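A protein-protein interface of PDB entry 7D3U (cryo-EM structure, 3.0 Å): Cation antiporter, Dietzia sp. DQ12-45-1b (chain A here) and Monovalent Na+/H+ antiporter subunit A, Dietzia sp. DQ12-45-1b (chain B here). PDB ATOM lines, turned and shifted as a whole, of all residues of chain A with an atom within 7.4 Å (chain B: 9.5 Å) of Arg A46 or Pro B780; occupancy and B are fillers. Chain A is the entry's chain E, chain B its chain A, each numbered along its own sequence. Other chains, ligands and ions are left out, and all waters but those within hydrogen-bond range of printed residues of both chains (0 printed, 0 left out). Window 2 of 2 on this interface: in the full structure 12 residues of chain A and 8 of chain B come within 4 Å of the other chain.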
ATOM      1  N   PHE A  44     -28.207  -0.729  14.022  1.00  0.00           N
ATOM      2  CA  PHE A  44     -28.394  -1.396  12.744  1.00  0.00           C
ATOM      3  C   PHE A  44     -28.697  -2.869  12.969  1.00  0.00           C
ATOM      4  O   PHE A  44     -28.231  -3.477  13.934  1.00  0.00           O
ATOM      5  CB  PHE A  44     -27.154  -1.244  11.866  1.00  0.00           C
ATOM      6  CG  PHE A  44     -26.799   0.179  11.560  1.00  0.00           C
ATOM      7  CD1 PHE A  44     -26.078   0.937  12.464  1.00  0.00           C
ATOM      8  CD2 PHE A  44     -27.185   0.761  10.368  1.00  0.00           C
ATOM      9  CE1 PHE A  44     -25.750   2.245  12.187  1.00  0.00           C
ATOM     10  CE2 PHE A  44     -26.857   2.069  10.087  1.00  0.00           C
ATOM     11  CZ  PHE A  44     -26.139   2.811  10.997  1.00  0.00           C
ATOM     12  N   VAL A  45     -29.479  -3.444  12.060  1.00  0.00           N
ATOM     13  CA  VAL A  45     -29.942  -4.819  12.208  1.00  0.00           C
ATOM     14  C   VAL A  45     -30.079  -5.439  10.826  1.00  0.00           C
ATOM     15  O   VAL A  45     -30.662  -4.837   9.920  1.00  0.00           O
ATOM     16  CB  VAL A  45     -31.283  -4.883  12.970  1.00  0.00           C
ATOM     17  CG1 VAL A  45     -31.815  -6.304  13.010  1.00  0.00           C
ATOM     18  CG2 VAL A  45     -31.121  -4.342  14.376  1.00  0.00           C
ATOM     19  N   ARG A  46     -29.532  -6.639  10.662  1.00  0.00           N
ATOM     20  CA  ARG A  46     -29.781  -7.445   9.476  1.00  0.00           C
ATOM     21  C   ARG A  46     -31.049  -8.253   9.715  1.00  0.00           C
ATOM     22  O   ARG A  46     -31.141  -8.994  10.699  1.00  0.00           O
ATOM     23  CB  ARG A  46     -28.599  -8.362   9.176  1.00  0.00           C
ATOM     24  CG  ARG A  46     -27.288  -7.627   9.013  1.00  0.00           C
ATOM     25  CD  ARG A  46     -26.145  -8.577   8.719  1.00  0.00           C
ATOM     26  NE  ARG A  46     -26.278  -9.195   7.404  1.00  0.00           N
ATOM     27  CZ  ARG A  46     -25.250  -9.559   6.647  1.00  0.00           C
ATOM     28  NH1 ARG A  46     -25.461 -10.115   5.463  1.00  0.00           N
ATOM     29  NH2 ARG A  46     -24.010  -9.363   7.072  1.00  0.00           N
ATOM     30  N   PHE A  47     -32.022  -8.108   8.821  1.00  0.00           N
ATOM     31  CA  PHE A  47     -33.341  -8.693   9.010  1.00  0.00           C
ATOM     32  C   PHE A  47     -33.678  -9.594   7.830  1.00  0.00           C
ATOM     33  O   PHE A  47     -33.734  -9.109   6.687  1.00  0.00           O
ATOM     34  CB  PHE A  47     -34.390  -7.589   9.159  1.00  0.00           C
ATOM     35  CG  PHE A  47     -35.785  -8.097   9.354  1.00  0.00           C
ATOM     36  CD1 PHE A  47     -36.044  -9.124  10.241  1.00  0.00           C
ATOM     37  CD2 PHE A  47     -36.840  -7.541   8.657  1.00  0.00           C
ATOM     38  CE1 PHE A  47     -37.330  -9.591  10.425  1.00  0.00           C
ATOM     39  CE2 PHE A  47     -38.125  -8.003   8.835  1.00  0.00           C
ATOM     40  CZ  PHE A  47     -38.371  -9.029   9.721  1.00  0.00           C
ATOM     41  N   PRO A  48     -33.885 -10.893   8.039  1.00  0.00           N
ATOM     42  CA  PRO A  48     -34.401 -11.740   6.956  1.00  0.00           C
ATOM     43  C   PRO A  48     -35.857 -11.398   6.678  1.00  0.00           C
ATOM     44  O   PRO A  48     -36.688 -11.380   7.587  1.00  0.00           O
ATOM     45  CB  PRO A  48     -34.243 -13.163   7.506  1.00  0.00           C
ATOM     46  CG  PRO A  48     -33.281 -13.034   8.655  1.00  0.00           C
ATOM     47  CD  PRO A  48     -33.529 -11.680   9.229  1.00  0.00           C
ATOM     48  N   THR A  49     -36.163 -11.134   5.410  1.00  0.00           N
ATOM     49  CA  THR A  49     -37.417 -10.478   5.066  1.00  0.00           C
ATOM     50  C   THR A  49     -38.550 -11.451   4.778  1.00  0.00           C
ATOM     51  O   THR A  49     -39.720 -11.088   4.946  1.00  0.00           O
ATOM     52  CB  THR A  49     -37.214  -9.564   3.855  1.00  0.00           C
ATOM     53  OG1 THR A  49     -36.249  -8.558   4.178  1.00  0.00           O
ATOM     54  CG2 THR A  49     -38.515  -8.874   3.497  1.00  0.00           C
ATOM     55  N   GLY A  74     -30.546  -0.793   2.950  1.00  0.00           N
ATOM     56  CA  GLY A  74     -30.442  -1.486   1.683  1.00  0.00           C
ATOM     57  C   GLY A  74     -30.953  -2.904   1.799  1.00  0.00           C
ATOM     58  O   GLY A  74     -31.378  -3.354   2.864  1.00  0.00           O
ATOM     59  N   ALA A  75     -30.910  -3.608   0.671  1.00  0.00           N
ATOM     60  CA  ALA A  75     -31.400  -4.973   0.593  1.00  0.00           C
ATOM     61  C   ALA A  75     -30.430  -5.821  -0.213  1.00  0.00           C
ATOM     62  O   ALA A  75     -29.799  -5.345  -1.159  1.00  0.00           O
ATOM     63  CB  ALA A  75     -32.795  -5.037  -0.036  1.00  0.00           C
ATOM     64  N   HIS A  76     -30.327  -7.088   0.176  1.00  0.00           N
ATOM     65  CA  HIS A  76     -29.498  -8.085  -0.487  1.00  0.00           C
ATOM     66  C   HIS A  76     -29.816  -9.436   0.127  1.00  0.00           C
ATOM     67  O   HIS A  76     -30.239  -9.514   1.284  1.00  0.00           O
ATOM     68  CB  HIS A  76     -28.005  -7.779  -0.339  1.00  0.00           C
ATOM     69  CG  HIS A  76     -27.319  -8.624   0.688  1.00  0.00           C
ATOM     70  ND1 HIS A  76     -27.579  -8.514   2.037  1.00  0.00           N
ATOM     71  CD2 HIS A  76     -26.387  -9.598   0.563  1.00  0.00           C
ATOM     72  CE1 HIS A  76     -26.833  -9.381   2.698  1.00  0.00           C
ATOM     73  NE2 HIS A  76     -26.101 -10.051   1.827  1.00  0.00           N
ATOM     74  N   HIS A  77     -29.600 -10.494  -0.645  1.00  0.00           N
ATOM     75  CA  HIS A  77     -29.867 -11.856  -0.190  1.00  0.00           C
ATOM     76  C   HIS A  77     -28.660 -12.737  -0.473  1.00  0.00           C
ATOM     77  O   HIS A  77     -28.399 -13.063  -1.650  1.00  0.00           O
ATOM     78  CB  HIS A  77     -31.117 -12.430  -0.852  1.00  0.00           C
ATOM     79  CG  HIS A  77     -31.221 -12.141  -2.317  1.00  0.00           C
ATOM     80  ND1 HIS A  77     -31.194 -13.134  -3.272  1.00  0.00           N
ATOM     81  CD2 HIS A  77     -31.375 -10.977  -2.990  1.00  0.00           C
ATOM     82  CE1 HIS A  77     -31.314 -12.594  -4.470  1.00  0.00           C
ATOM     83  NE2 HIS A  77     -31.424 -11.285  -4.327  1.00  0.00           N
ATOM     84  N   PRO A  78     -27.903 -13.145   0.552  1.00  0.00           N
ATOM     85  CA  PRO A  78     -26.759 -14.047   0.364  1.00  0.00           C
ATOM     86  C   PRO A  78     -27.167 -15.514   0.256  1.00  0.00           C
ATOM     87  O   PRO A  78     -26.578 -16.392   0.888  1.00  0.00           O
ATOM     88  CB  PRO A  78     -25.917 -13.783   1.616  1.00  0.00           C
ATOM     89  CG  PRO A  78     -26.931 -13.472   2.660  1.00  0.00           C
ATOM     90  CD  PRO A  78     -28.068 -12.758   1.964  1.00  0.00           C
ATOM     91  N   GLU A  85     -32.829 -10.241   2.351  1.00  0.00           N
ATOM     92  CA  GLU A  85     -32.415  -9.643   3.610  1.00  0.00           C
ATOM     93  C   GLU A  85     -32.388  -8.129   3.463  1.00  0.00           C
ATOM     94  O   GLU A  85     -32.094  -7.602   2.389  1.00  0.00           O
ATOM     95  CB  GLU A  85     -31.030 -10.140   4.034  1.00  0.00           C
ATOM     96  CG  GLU A  85     -31.045 -11.326   4.975  1.00  0.00           C
ATOM     97  CD  GLU A  85     -29.728 -11.494   5.706  1.00  0.00           C
ATOM     98  OE1 GLU A  85     -28.851 -10.619   5.556  1.00  0.00           O
ATOM     99  OE2 GLU A  85     -29.570 -12.498   6.432  1.00  0.00           O
ATOM    100  N   ILE A  86     -32.704  -7.430   4.548  1.00  0.00           N
ATOM    101  CA  ILE A  86     -32.645  -5.976   4.554  1.00  0.00           C
ATOM    102  C   ILE A  86     -31.767  -5.522   5.711  1.00  0.00           C
ATOM    103  O   ILE A  86     -31.495  -6.268   6.652  1.00  0.00           O
ATOM    104  CB  ILE A  86     -34.040  -5.328   4.643  1.00  0.00           C
ATOM    105  CG1 ILE A  86     -34.799  -5.846   5.862  1.00  0.00           C
ATOM    106  CG2 ILE A  86     -34.828  -5.587   3.373  1.00  0.00           C
ATOM    107  CD1 ILE A  86     -36.239  -5.399   5.902  1.00  0.00           C
ATOM    108  N   VAL A  87     -31.311  -4.278   5.618  1.00  0.00           N
ATOM    109  CA  VAL A  87     -30.505  -3.647   6.655  1.00  0.00           C
ATOM    110  C   VAL A  87     -31.317  -2.485   7.201  1.00  0.00           C
ATOM    111  O   VAL A  87     -31.473  -1.458   6.528  1.00  0.00           O
ATOM    112  CB  VAL A  87     -29.150  -3.172   6.123  1.00  0.00           C
ATOM    113  CG1 VAL A  87     -28.385  -2.444   7.211  1.00  0.00           C
ATOM    114  CG2 VAL A  87     -28.353  -4.349   5.600  1.00  0.00           C
ATOM    115  N   VAL A  88     -31.835  -2.639   8.415  1.00  0.00           N
ATOM    116  CA  VAL A  88     -32.745  -1.674   9.016  1.00  0.00           C
ATOM    117  C   VAL A  88     -32.019  -0.935  10.127  1.00  0.00           C
ATOM    118  O   VAL A  88     -31.371  -1.554  10.977  1.00  0.00           O
ATOM    119  CB  VAL A  88     -34.011  -2.360   9.550  1.00  0.00           C
ATOM    120  CG1 VAL A  88     -34.994  -1.327  10.051  1.00  0.00           C
ATOM    121  CG2 VAL A  88     -34.636  -3.205   8.463  1.00  0.00           C
ATOM    122  N   LEU A  99     -36.259  -4.468  18.077  1.00  0.00           N
ATOM    123  CA  LEU A  99     -36.350  -3.978  16.707  1.00  0.00           C
ATOM    124  C   LEU A  99     -36.814  -5.078  15.762  1.00  0.00           C
ATOM    125  O   LEU A  99     -37.708  -4.865  14.937  1.00  0.00           O
ATOM    126  CB  LEU A  99     -34.995  -3.418  16.270  1.00  0.00           C
ATOM    127  CG  LEU A  99     -34.904  -2.811  14.872  1.00  0.00           C
ATOM    128  CD1 LEU A  99     -36.047  -1.847  14.647  1.00  0.00           C
ATOM    129  CD2 LEU A  99     -33.570  -2.113  14.681  1.00  0.00           C
ATOM    130  N   THR A 100     -36.223  -6.271  15.876  1.00  0.00           N
ATOM    131  CA  THR A 100     -36.629  -7.371  15.011  1.00  0.00           C
ATOM    132  C   THR A 100     -38.059  -7.815  15.288  1.00  0.00           C
ATOM    133  O   THR A 100     -38.763  -8.216  14.360  1.00  0.00           O
ATOM    134  CB  THR A 100     -35.680  -8.557  15.158  1.00  0.00           C
ATOM    135  OG1 THR A 100     -35.797  -9.103  16.479  1.00  0.00           O
ATOM    136  CG2 THR A 100     -34.244  -8.141  14.885  1.00  0.00           C
ATOM    137  N   LEU A 103     -40.237  -5.283  13.546  1.00  0.00           N
ATOM    138  CA  LEU A 103     -40.167  -5.491  12.104  1.00  0.00           C
ATOM    139  C   LEU A 103     -40.929  -6.740  11.686  1.00  0.00           C
ATOM    140  O   LEU A 103     -41.550  -6.763  10.621  1.00  0.00           O
ATOM    141  CB  LEU A 103     -38.713  -5.580  11.652  1.00  0.00           C
ATOM    142  CG  LEU A 103     -37.869  -4.333  11.895  1.00  0.00           C
ATOM    143  CD1 LEU A 103     -36.523  -4.480  11.221  1.00  0.00           C
ATOM    144  CD2 LEU A 103     -38.591  -3.086  11.418  1.00  0.00           C
ATOM    145  N   ALA B 774     -15.053   2.680   1.547  1.00  0.00           N
ATOM    146  CA  ALA B 774     -14.479   2.099   2.760  1.00  0.00           C
ATOM    147  C   ALA B 774     -15.455   1.113   3.404  1.00  0.00           C
ATOM    148  O   ALA B 774     -15.860   1.249   4.558  1.00  0.00           O
ATOM    149  CB  ALA B 774     -14.081   3.203   3.733  1.00  0.00           C
ATOM    150  N   VAL B 775     -15.831   0.105   2.622  1.00  0.00           N
ATOM    151  CA  VAL B 775     -16.652  -1.007   3.090  1.00  0.00           C
ATOM    152  C   VAL B 775     -16.111  -2.284   2.464  1.00  0.00           C
ATOM    153  O   VAL B 775     -15.695  -2.288   1.301  1.00  0.00           O
ATOM    154  CB  VAL B 775     -18.147  -0.815   2.750  1.00  0.00           C
ATOM    155  CG1 VAL B 775     -18.716   0.387   3.481  1.00  0.00           C
ATOM    156  CG2 VAL B 775     -18.341  -0.657   1.251  1.00  0.00           C
ATOM    157  N   HIS B 776     -16.098  -3.365   3.238  1.00  0.00           N
ATOM    158  CA  HIS B 776     -15.556  -4.606   2.712  1.00  0.00           C
ATOM    159  C   HIS B 776     -16.590  -5.311   1.835  1.00  0.00           C
ATOM    160  O   HIS B 776     -17.771  -4.956   1.804  1.00  0.00           O
ATOM    161  CB  HIS B 776     -15.066  -5.508   3.845  1.00  0.00           C
ATOM    162  CG  HIS B 776     -16.152  -6.015   4.740  1.00  0.00           C
ATOM    163  ND1 HIS B 776     -16.262  -5.635   6.060  1.00  0.00           N
ATOM    164  CD2 HIS B 776     -17.158  -6.894   4.517  1.00  0.00           C
ATOM    165  CE1 HIS B 776     -17.297  -6.246   6.607  1.00  0.00           C
ATOM    166  NE2 HIS B 776     -17.858  -7.015   5.692  1.00  0.00           N
ATOM    167  N   ALA B 777     -16.123  -6.331   1.113  1.00  0.00           N
ATOM    168  CA  ALA B 777     -16.902  -6.891   0.013  1.00  0.00           C
ATOM    169  C   ALA B 777     -18.123  -7.656   0.512  1.00  0.00           C
ATOM    170  O   ALA B 777     -19.230  -7.483  -0.011  1.00  0.00           O
ATOM    171  CB  ALA B 777     -16.018  -7.795  -0.844  1.00  0.00           C
ATOM    172  N   ASP B 778     -17.947  -8.504   1.521  1.00  0.00           N
ATOM    173  CA  ASP B 778     -19.002  -9.422   1.933  1.00  0.00           C
ATOM    174  C   ASP B 778     -20.124  -8.744   2.710  1.00  0.00           C
ATOM    175  O   ASP B 778     -20.971  -9.443   3.274  1.00  0.00           O
ATOM    176  CB  ASP B 778     -18.413 -10.563   2.768  1.00  0.00           C
ATOM    177  CG  ASP B 778     -17.695 -10.072   4.010  1.00  0.00           C
ATOM    178  OD1 ASP B 778     -18.377  -9.707   4.991  1.00  0.00           O
ATOM    179  OD2 ASP B 778     -16.447 -10.054   4.007  1.00  0.00           O
ATOM    180  N   SER B 779     -20.153  -7.422   2.754  1.00  0.00           N
ATOM    181  CA  SER B 779     -21.209  -6.785   3.520  1.00  0.00           C
ATOM    182  C   SER B 779     -22.336  -6.321   2.607  1.00  0.00           C
ATOM    183  O   SER B 779     -22.114  -6.040   1.426  1.00  0.00           O
ATOM    184  CB  SER B 779     -20.666  -5.582   4.297  1.00  0.00           C
ATOM    185  OG  SER B 779     -20.963  -4.370   3.627  1.00  0.00           O
ATOM    186  N   PRO B 780     -23.552  -6.226   3.132  1.00  0.00           N
ATOM    187  CA  PRO B 780     -24.649  -5.653   2.346  1.00  0.00           C
ATOM    188  C   PRO B 780     -24.454  -4.166   2.121  1.00  0.00           C
ATOM    189  O   PRO B 780     -23.403  -3.617   2.467  1.00  0.00           O
ATOM    190  CB  PRO B 780     -25.887  -5.946   3.200  1.00  0.00           C
ATOM    191  CG  PRO B 780     -25.365  -6.104   4.571  1.00  0.00           C
ATOM    192  CD  PRO B 780     -24.015  -6.728   4.435  1.00  0.00           C
ATOM    193  N   LEU B 781     -25.452  -3.514   1.525  1.00  0.00           N
ATOM    194  CA  LEU B 781     -25.362  -2.138   1.043  1.00  0.00           C
ATOM    195  C   LEU B 781     -24.370  -2.007  -0.105  1.00  0.00           C
ATOM    196  O   LEU B 781     -23.951  -0.900  -0.448  1.00  0.00           O
ATOM    197  CB  LEU B 781     -25.013  -1.155   2.168  1.00  0.00           C
ATOM    198  CG  LEU B 781     -25.795  -1.322   3.475  1.00  0.00           C
ATOM    199  CD1 LEU B 781     -25.608  -0.133   4.382  1.00  0.00           C
ATOM    200  CD2 LEU B 781     -27.265  -1.522   3.201  1.00  0.00           C
ATOM    201  N   LEU B 782     -23.984  -3.138  -0.689  1.00  0.00           N
ATOM    202  CA  LEU B 782     -23.190  -3.213  -1.906  1.00  0.00           C
ATOM    203  C   LEU B 782     -23.941  -4.108  -2.880  1.00  0.00           C
ATOM    204  O   LEU B 782     -25.112  -4.422  -2.641  1.00  0.00           O
ATOM    205  CB  LEU B 782     -21.786  -3.750  -1.623  1.00  0.00           C
ATOM    206  CG  LEU B 782     -20.663  -2.719  -1.649  1.00  0.00           C
ATOM    207  CD1 LEU B 782     -19.319  -3.407  -1.515  1.00  0.00           C
ATOM    208  CD2 LEU B 782     -20.729  -1.922  -2.934  1.00  0.00           C
ATOM    209  N   SER B 783     -23.299  -4.516  -3.974  1.00  0.00           N
ATOM    210  CA  SER B 783     -23.919  -5.388  -4.970  1.00  0.00           C
ATOM    211  C   SER B 783     -25.146  -4.707  -5.584  1.00  0.00           C
ATOM    212  O   SER B 783     -26.294  -5.124  -5.404  1.00  0.00           O
ATOM    213  CB  SER B 783     -24.281  -6.748  -4.361  1.00  0.00           C
ATOM    214  OG  SER B 783     -25.260  -6.610  -3.348  1.00  0.00           O
ATOM    215  N   ALA B 784     -24.849  -3.614  -6.293  1.00  0.00           N
ATOM    216  CA  ALA B 784     -25.885  -2.741  -6.842  1.00  0.00           C
ATOM    217  C   ALA B 784     -26.986  -3.507  -7.565  1.00  0.00           C
ATOM    218  O   ALA B 784     -28.147  -3.092  -7.532  1.00  0.00           O
ATOM    219  CB  ALA B 784     -25.250  -1.725  -7.789  1.00  0.00           C
ATOM    220  N   ASP B 786     -28.295  -6.285  -6.691  1.00  0.00           N
ATOM    221  CA  ASP B 786     -29.200  -6.763  -5.656  1.00  0.00           C
ATOM    222  C   ASP B 786     -29.695  -5.656  -4.737  1.00  0.00           C
ATOM    223  O   ASP B 786     -30.653  -5.879  -3.991  1.00  0.00           O
ATOM    224  CB  ASP B 786     -28.512  -7.845  -4.817  1.00  0.00           C
ATOM    225  CG  ASP B 786     -28.883  -9.243  -5.257  1.00  0.00           C
ATOM    226  OD1 ASP B 786     -29.761  -9.374  -6.137  1.00  0.00           O
ATOM    227  OD2 ASP B 786     -28.299 -10.210  -4.726  1.00  0.00           O
ATOM    228  N   ASN B 787     -29.078  -4.476  -4.775  1.00  0.00           N
ATOM    229  CA  ASN B 787     -29.417  -3.398  -3.859  1.00  0.00           C
ATOM    230  C   ASN B 787     -30.195  -2.265  -4.508  1.00  0.00           C
ATOM    231  O   ASN B 787     -30.672  -1.378  -3.794  1.00  0.00           O
ATOM    232  CB  ASN B 787     -28.145  -2.831  -3.217  1.00  0.00           C
ATOM    233  CG  ASN B 787     -28.418  -2.152  -1.897  1.00  0.00           C
ATOM    234  OD1 ASN B 787     -29.473  -2.345  -1.297  1.00  0.00           O
ATOM    235  ND2 ASN B 787     -27.468  -1.354  -1.434  1.00  0.00           N
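The side-chain carboxylate of Asp B786 is in hydrogen-bond range of a ring nitrogen (NE2) of His A77, at 3.1 Å. The backbone NH (N) of Ala A75 is in hydrogen-bond range of the side-chain amide oxygen (OD1) of Asn B787 (2.7 Å). The backbone carbonyl oxygen (O) of Ala A75 lies close to the backbone carbonyl oxygen (O) of Asp B786, 3.0 Å away.
The guanidinium group of Arg A46 lies within salt-bridge range of the side-chain carboxylate of Glu A85 (3.4 Å). The backbone NH (N) of Val A87 sits at hydrogen-bond distance from the backbone carbonyl oxygen (O) of Gly A74, at 2.9 Å. The backbone carbonyl oxygen (O) of Glu A85 lies within hydrogen-bond range of the backbone NH (N) of His A76, at 2.9 Å.
Arg A46 touches Pro B780 (NH2 to CD, 3.7 Å). Gly A74 touches Leu B781. Gly A74 touches Asn B787 (CA to OD1, 3.2 Å). Pro B780 touches His A76 (CB to ND1, 3.3 Å). Val A87 touches Pro B780 (CG2 to CG, 3.6 Å). Val A87 touches Leu B781.
No residue of chain B comes within 4 Å of Val A45. Printed residues of chain B within 4 Å of Arg A46: Pro B780. Of the printed residues of chain B, Gly A74 touches Leu B781 and Asn B787. Of the printed residues of chain B, Ala A75 touches Asp B786 and Asn B787. Val B775 touches none of the printed residues of chain A. Ala B777 touches none of the printed residues of chain A. Of chain A, only Arg A46 (3.7 Å), His A76 (3.3 Å) and Val A87 (3.6 Å) come within 4 Å of Pro B780. Of the printed residues of chain A, Leu B781 touches Gly A74 (3.4 Å) and Val A87 (3.8 Å). Of the printed residues of chain A, Asp B786 touches Ala A75 and His A77. Of the printed residues of chain A, Asn B787 touches Gly A74 and Ala A75. The nearest residue of chain B that does not touch Arg A46 is Asp B778 (4.9 Å). The nearest residue of chain A that does not touch Pro B780 is Ala A75 (5.7 Å). The nearest printed residue of chain B that does not touch Val A87 is Ser B779 (7.0 Å).
Printed residues of chain B that touch a printed residue of chain A: Pro B780, Leu B781, Asp B786 and Asn B787. Hydrophobic or aromatic side chains of chain B that line the printed part of chain A: Pro B780 and Leu B781. Along chain B the printed residues that touch a printed residue of chain A span positions 780 to 787. Among the printed residues, no Asp or Glu carboxylate lies within 4 Å of a Lys or Arg side-chain nitrogen of the other chain.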
